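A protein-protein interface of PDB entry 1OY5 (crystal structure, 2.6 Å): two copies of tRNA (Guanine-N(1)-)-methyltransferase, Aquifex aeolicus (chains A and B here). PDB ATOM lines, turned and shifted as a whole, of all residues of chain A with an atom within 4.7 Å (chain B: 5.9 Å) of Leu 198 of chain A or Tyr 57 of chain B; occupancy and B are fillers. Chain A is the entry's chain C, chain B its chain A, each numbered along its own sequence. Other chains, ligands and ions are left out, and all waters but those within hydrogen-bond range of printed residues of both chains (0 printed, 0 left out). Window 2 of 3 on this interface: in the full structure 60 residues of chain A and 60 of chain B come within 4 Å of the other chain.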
ATOM      1  N   TYR A 182       3.327 -28.054  11.934  1.00  0.00           N
ATOM      2  CA  TYR A 182       3.656 -28.521  10.593  1.00  0.00           C
ATOM      3  C   TYR A 182       4.770 -29.537  10.630  1.00  0.00           C
ATOM      4  O   TYR A 182       5.537 -29.592  11.579  1.00  0.00           O
ATOM      5  CB  TYR A 182       4.132 -27.384   9.718  1.00  0.00           C
ATOM      6  CG  TYR A 182       3.063 -26.426   9.327  1.00  0.00           C
ATOM      7  CD1 TYR A 182       2.464 -26.500   8.079  1.00  0.00           C
ATOM      8  CD2 TYR A 182       2.663 -25.426  10.190  1.00  0.00           C
ATOM      9  CE1 TYR A 182       1.485 -25.619   7.705  1.00  0.00           C
ATOM     10  CE2 TYR A 182       1.683 -24.549   9.832  1.00  0.00           C
ATOM     11  CZ  TYR A 182       1.093 -24.645   8.589  1.00  0.00           C
ATOM     12  OH  TYR A 182       0.122 -23.725   8.234  1.00  0.00           O
ATOM     13  N   THR A 183       4.862 -30.331   9.574  1.00  0.00           N
ATOM     14  CA  THR A 183       5.903 -31.328   9.510  1.00  0.00           C
ATOM     15  C   THR A 183       6.552 -31.479   8.166  1.00  0.00           C
ATOM     16  O   THR A 183       6.108 -30.926   7.183  1.00  0.00           O
ATOM     17  CB  THR A 183       5.436 -32.665  10.030  1.00  0.00           C
ATOM     18  OG1 THR A 183       6.590 -33.456  10.319  1.00  0.00           O
ATOM     19  CG2 THR A 183       4.617 -33.459   9.002  1.00  0.00           C
ATOM     20  N   ARG A 184       7.595 -32.299   8.174  1.00  0.00           N
ATOM     21  CA  ARG A 184       8.589 -32.384   7.106  1.00  0.00           C
ATOM     22  C   ARG A 184       8.223 -31.985   5.722  1.00  0.00           C
ATOM     23  O   ARG A 184       8.837 -31.057   5.149  1.00  0.00           O
ATOM     24  CB  ARG A 184       9.196 -33.749   7.028  1.00  0.00           C
ATOM     25  CG  ARG A 184      10.615 -33.651   6.569  1.00  0.00           C
ATOM     26  CD  ARG A 184      11.584 -33.299   7.689  1.00  0.00           C
ATOM     27  NE  ARG A 184      11.131 -32.246   8.596  1.00  0.00           N
ATOM     28  CZ  ARG A 184      11.953 -31.601   9.421  1.00  0.00           C
ATOM     29  NH1 ARG A 184      13.237 -31.918   9.438  1.00  0.00           N
ATOM     30  NH2 ARG A 184      11.507 -30.656  10.236  1.00  0.00           N
ATOM     31  N   PRO A 185       7.252 -32.645   5.138  1.00  0.00           N
ATOM     32  CA  PRO A 185       6.962 -32.301   3.764  1.00  0.00           C
ATOM     33  C   PRO A 185       6.952 -30.766   3.762  1.00  0.00           C
ATOM     34  O   PRO A 185       6.071 -30.128   4.337  1.00  0.00           O
ATOM     35  CB  PRO A 185       5.615 -32.951   3.542  1.00  0.00           C
ATOM     36  CG  PRO A 185       5.684 -34.113   4.492  1.00  0.00           C
ATOM     37  CD  PRO A 185       6.327 -33.630   5.700  1.00  0.00           C
ATOM     38  N   ARG A 186       7.982 -30.171   3.181  1.00  0.00           N
ATOM     39  CA  ARG A 186       8.111 -28.707   3.132  1.00  0.00           C
ATOM     40  C   ARG A 186       7.026 -28.058   2.294  1.00  0.00           C
ATOM     41  O   ARG A 186       6.512 -26.987   2.628  1.00  0.00           O
ATOM     42  CB  ARG A 186       9.462 -28.341   2.564  1.00  0.00           C
ATOM     43  CG  ARG A 186       9.685 -26.860   2.483  1.00  0.00           C
ATOM     44  CD  ARG A 186      10.894 -26.501   1.665  1.00  0.00           C
ATOM     45  NE  ARG A 186      11.017 -25.065   1.440  1.00  0.00           N
ATOM     46  CZ  ARG A 186      10.104 -24.305   0.833  1.00  0.00           C
ATOM     47  NH1 ARG A 186       8.962 -24.824   0.375  1.00  0.00           N
ATOM     48  NH2 ARG A 186      10.344 -23.002   0.686  1.00  0.00           N
ATOM     49  N   VAL A 193       4.764 -24.937   3.934  1.00  0.00           N
ATOM     50  CA  VAL A 193       4.907 -24.613   5.336  1.00  0.00           C
ATOM     51  C   VAL A 193       5.282 -23.149   5.454  1.00  0.00           C
ATOM     52  O   VAL A 193       5.997 -22.620   4.609  1.00  0.00           O
ATOM     53  CB  VAL A 193       5.981 -25.473   5.996  1.00  0.00           C
ATOM     54  CG1 VAL A 193       6.199 -25.049   7.436  1.00  0.00           C
ATOM     55  CG2 VAL A 193       5.581 -26.932   5.937  1.00  0.00           C
ATOM     56  N   PRO A 194       4.761 -22.482   6.475  1.00  0.00           N
ATOM     57  CA  PRO A 194       5.126 -21.098   6.737  1.00  0.00           C
ATOM     58  C   PRO A 194       6.635 -20.940   6.874  1.00  0.00           C
ATOM     59  O   PRO A 194       7.252 -21.447   7.818  1.00  0.00           O
ATOM     60  CB  PRO A 194       4.420 -20.803   8.057  1.00  0.00           C
ATOM     61  CG  PRO A 194       3.270 -21.732   8.075  1.00  0.00           C
ATOM     62  CD  PRO A 194       3.758 -22.972   7.434  1.00  0.00           C
ATOM     63  N   GLU A 195       7.213 -20.246   5.898  1.00  0.00           N
ATOM     64  CA  GLU A 195       8.638 -19.903   5.862  1.00  0.00           C
ATOM     65  C   GLU A 195       9.190 -19.433   7.206  1.00  0.00           C
ATOM     66  O   GLU A 195      10.380 -19.547   7.458  1.00  0.00           O
ATOM     67  CB  GLU A 195       8.883 -18.822   4.812  1.00  0.00           C
ATOM     68  CG  GLU A 195       7.618 -18.135   4.298  1.00  0.00           C
ATOM     69  CD  GLU A 195       6.873 -17.333   5.359  1.00  0.00           C
ATOM     70  OE1 GLU A 195       6.442 -17.938   6.373  1.00  0.00           O
ATOM     71  OE2 GLU A 195       6.715 -16.093   5.166  1.00  0.00           O
ATOM     72  N   GLU A 196       8.331 -18.889   8.055  1.00  0.00           N
ATOM     73  CA  GLU A 196       8.732 -18.524   9.397  1.00  0.00           C
ATOM     74  C   GLU A 196       9.352 -19.730  10.073  1.00  0.00           C
ATOM     75  O   GLU A 196      10.535 -19.736  10.388  1.00  0.00           O
ATOM     76  CB  GLU A 196       7.520 -18.066  10.193  1.00  0.00           C
ATOM     77  CG  GLU A 196       6.853 -16.842   9.600  1.00  0.00           C
ATOM     78  CD  GLU A 196       5.547 -16.505  10.273  1.00  0.00           C
ATOM     79  OE1 GLU A 196       4.639 -17.345  10.202  1.00  0.00           O
ATOM     80  OE2 GLU A 196       5.428 -15.401  10.847  1.00  0.00           O
ATOM     81  N   LEU A 197       8.544 -20.768  10.259  1.00  0.00           N
ATOM     82  CA  LEU A 197       8.969 -21.992  10.917  1.00  0.00           C
ATOM     83  C   LEU A 197      10.230 -22.673  10.331  1.00  0.00           C
ATOM     84  O   LEU A 197      10.778 -23.565  10.967  1.00  0.00           O
ATOM     85  CB  LEU A 197       7.791 -22.972  10.936  1.00  0.00           C
ATOM     86  CG  LEU A 197       6.521 -22.478  11.649  1.00  0.00           C
ATOM     87  CD1 LEU A 197       5.421 -23.519  11.583  1.00  0.00           C
ATOM     88  CD2 LEU A 197       6.787 -22.125  13.103  1.00  0.00           C
ATOM     89  N   LEU A 198      10.725 -22.244   9.168  1.00  0.00           N
ATOM     90  CA  LEU A 198      11.839 -22.961   8.497  1.00  0.00           C
ATOM     91  C   LEU A 198      13.293 -22.576   8.715  1.00  0.00           C
ATOM     92  O   LEU A 198      14.200 -23.398   8.587  1.00  0.00           O
ATOM     93  CB  LEU A 198      11.615 -22.925   6.999  1.00  0.00           C
ATOM     94  CG  LEU A 198      10.296 -23.597   6.654  1.00  0.00           C
ATOM     95  CD1 LEU A 198      10.004 -23.422   5.195  1.00  0.00           C
ATOM     96  CD2 LEU A 198      10.303 -25.084   7.035  1.00  0.00           C
ATOM     97  N   SER A 199      13.524 -21.319   8.982  1.00  0.00           N
ATOM     98  CA  SER A 199      14.844 -20.825   9.185  1.00  0.00           C
ATOM     99  C   SER A 199      14.650 -20.434  10.611  1.00  0.00           C
ATOM    100  O   SER A 199      13.566 -20.656  11.127  1.00  0.00           O
ATOM    101  CB  SER A 199      14.924 -19.602   8.332  1.00  0.00           C
ATOM    102  OG  SER A 199      13.783 -18.830   8.651  1.00  0.00           O
ATOM    103  N   GLY A 200      15.594 -19.814  11.285  1.00  0.00           N
ATOM    104  CA  GLY A 200      15.151 -19.336  12.570  1.00  0.00           C
ATOM    105  C   GLY A 200      16.020 -18.930  13.718  1.00  0.00           C
ATOM    106  O   GLY A 200      15.500 -18.728  14.816  1.00  0.00           O
ATOM    107  N   VAL B  55       9.159 -35.009  12.413  1.00  0.00           N
ATOM    108  CA  VAL B  55       9.501 -33.907  13.308  1.00  0.00           C
ATOM    109  C   VAL B  55       8.908 -32.611  12.776  1.00  0.00           C
ATOM    110  O   VAL B  55       9.013 -32.311  11.594  1.00  0.00           O
ATOM    111  CB  VAL B  55      11.020 -33.735  13.433  1.00  0.00           C
ATOM    112  CG1 VAL B  55      11.353 -32.680  14.479  1.00  0.00           C
ATOM    113  CG2 VAL B  55      11.671 -35.038  13.809  1.00  0.00           C
ATOM    114  N   PRO B  56       8.246 -31.860  13.639  1.00  0.00           N
ATOM    115  CA  PRO B  56       7.643 -30.593  13.240  1.00  0.00           C
ATOM    116  C   PRO B  56       8.659 -29.486  13.050  1.00  0.00           C
ATOM    117  O   PRO B  56       9.812 -29.661  13.413  1.00  0.00           O
ATOM    118  CB  PRO B  56       6.701 -30.294  14.404  1.00  0.00           C
ATOM    119  CG  PRO B  56       7.328 -30.934  15.550  1.00  0.00           C
ATOM    120  CD  PRO B  56       7.909 -32.202  15.028  1.00  0.00           C
ATOM    121  N   TYR B  57       8.250 -28.365  12.471  1.00  0.00           N
ATOM    122  CA  TYR B  57       9.170 -27.256  12.241  1.00  0.00           C
ATOM    123  C   TYR B  57       9.068 -26.284  13.390  1.00  0.00           C
ATOM    124  O   TYR B  57       8.241 -26.449  14.275  1.00  0.00           O
ATOM    125  CB  TYR B  57       8.839 -26.548  10.949  1.00  0.00           C
ATOM    126  CG  TYR B  57       9.193 -27.348   9.725  1.00  0.00           C
ATOM    127  CD1 TYR B  57       8.200 -27.961   8.955  1.00  0.00           C
ATOM    128  CD2 TYR B  57      10.514 -27.490   9.326  1.00  0.00           C
ATOM    129  CE1 TYR B  57       8.520 -28.690   7.823  1.00  0.00           C
ATOM    130  CE2 TYR B  57      10.841 -28.217   8.199  1.00  0.00           C
ATOM    131  CZ  TYR B  57       9.835 -28.824   7.455  1.00  0.00           C
ATOM    132  OH  TYR B  57      10.142 -29.556   6.331  1.00  0.00           O
ATOM    133  N   GLY B  58       9.922 -25.277  13.393  1.00  0.00           N
ATOM    134  CA  GLY B  58       9.921 -24.314  14.469  1.00  0.00           C
ATOM    135  C   GLY B  58      10.399 -24.949  15.756  1.00  0.00           C
ATOM    136  O   GLY B  58      10.202 -24.385  16.835  1.00  0.00           O
ATOM    137  N   GLY B  59      11.021 -26.121  15.637  1.00  0.00           N
ATOM    138  CA  GLY B  59      11.584 -26.816  16.778  1.00  0.00           C
ATOM    139  C   GLY B  59      10.592 -27.020  17.902  1.00  0.00           C
ATOM    140  O   GLY B  59      10.379 -26.135  18.712  1.00  0.00           O
ATOM    141  N   LEU B  60       9.979 -28.194  17.944  1.00  0.00           N
ATOM    142  CA  LEU B  60       9.052 -28.542  19.006  1.00  0.00           C
ATOM    143  C   LEU B  60       9.424 -29.926  19.502  1.00  0.00           C
ATOM    144  O   LEU B  60      10.002 -30.706  18.756  1.00  0.00           O
ATOM    145  CB  LEU B  60       7.595 -28.535  18.501  1.00  0.00           C
ATOM    146  CG  LEU B  60       6.939 -27.146  18.469  1.00  0.00           C
ATOM    147  CD1 LEU B  60       7.116 -26.450  19.825  1.00  0.00           C
ATOM    148  CD2 LEU B  60       7.506 -26.268  17.351  1.00  0.00           C
ATOM    149  N   ARG B 123      -2.136 -28.369   7.140  1.00  0.00           N
ATOM    150  CA  ARG B 123      -2.618 -28.421   5.767  1.00  0.00           C
ATOM    151  C   ARG B 123      -3.730 -29.470   5.546  1.00  0.00           C
ATOM    152  O   ARG B 123      -4.390 -29.520   4.503  1.00  0.00           O
ATOM    153  CB  ARG B 123      -1.445 -28.657   4.822  1.00  0.00           C
ATOM    154  CG  ARG B 123      -0.464 -27.502   4.775  1.00  0.00           C
ATOM    155  CD  ARG B 123       0.898 -27.871   4.201  1.00  0.00           C
ATOM    156  NE  ARG B 123       1.642 -28.770   5.083  1.00  0.00           N
ATOM    157  CZ  ARG B 123       2.828 -29.315   4.795  1.00  0.00           C
ATOM    158  NH1 ARG B 123       3.435 -29.062   3.643  1.00  0.00           N
ATOM    159  NH2 ARG B 123       3.423 -30.105   5.672  1.00  0.00           N
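Along chain A the printed residues that touch a printed residue of chain B span positions 182 to 198. Of the 7 printed residues of chain B, 5 touch a printed residue of chain A. Printed residues of chain B that touch a printed residue of chain A: Val 55, Pro 56, Tyr 57, Gly 58 and Arg 123. Hydrophobic or aromatic side chains of chain B that line the printed part of chain A: Pro 56 and Tyr 57.
O of Tyr 182 of chain A touches CA of Pro 56 of chain B, at 2.9 Å. Arg 123 of chain B touches Tyr 182 of chain A. Thr 183 of chain A touches Tyr 57 of chain B. NH2 of Arg 184 of chain A touches O of Pro 56 of chain B, at 3.7 Å. N of Arg 186 of chain A touches OH of Tyr 57 of chain B (3.9 Å). Arg 123 of chain B touches Arg 186 of chain A (NH1 to O, 3.8 Å). Val 193 of chain A touches Tyr 57 of chain B. Val 193 of chain A touches Arg 123 of chain B. Tyr 57 of chain B touches Leu 197 of chain A. CD2 of Leu 198 of chain A touches CD2 of Tyr 57 of chain B, 3.3 Å away.
No position is printed for both chains. Of the 17 pairs that touch across the chains among the printed residues, none has its exchanged pair printed and touching as well.
The side-chain hydroxyl (OG1) of Thr 183 of chain A sits at hydrogen-bond distance from the backbone carbonyl oxygen (O) of Val 55 of chain B (3.0 Å). O of Val 55 of chain B lies within hydrogen-bond range of NH2 of Arg 184 of chain A (3.3 Å). The backbone carbonyl oxygen (O) of Tyr 182 of chain A lies within hydrogen-bond range of the backbone NH (N) of Tyr 57 of chain B (3.1 Å). The backbone carbonyl oxygen (O) of Leu 197 of chain A sits at hydrogen-bond distance from the backbone NH (N) of Gly 58 of chain B (3.1 Å). NH2 of Arg 123 of chain B sits at hydrogen-bond distance from O of Thr 183 of chain A (3.2 Å). The guanidinium group of Arg 123 of chain B sits at hydrogen-bond distance from the backbone carbonyl oxygen of Pro 185 of chain A (2.9 Å). O of Arg 184 of chain A lies close to OH of Tyr 57 of chain B.
The backbone carbonyl oxygen (O) of Arg 186 of chain A sits at hydrogen-bond distance from the backbone NH (N) of Val 193 of chain A (3.0 Å).
Of chain B, only Tyr 57 (3.3 Å) comes within 4 Å of Leu 198 of chain A. Of the printed residues of chain B, Leu 197 of chain A touches Tyr 57 and Gly 58. Printed residues of chain A within 4 Å of Gly 58 of chain B: Leu 197. Glu 196 of chain A touches none of the printed residues of chain B. The nearest residue of chain A that does not touch Tyr 57 of chain B is Pro 185 of chain A (4.3 Å).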
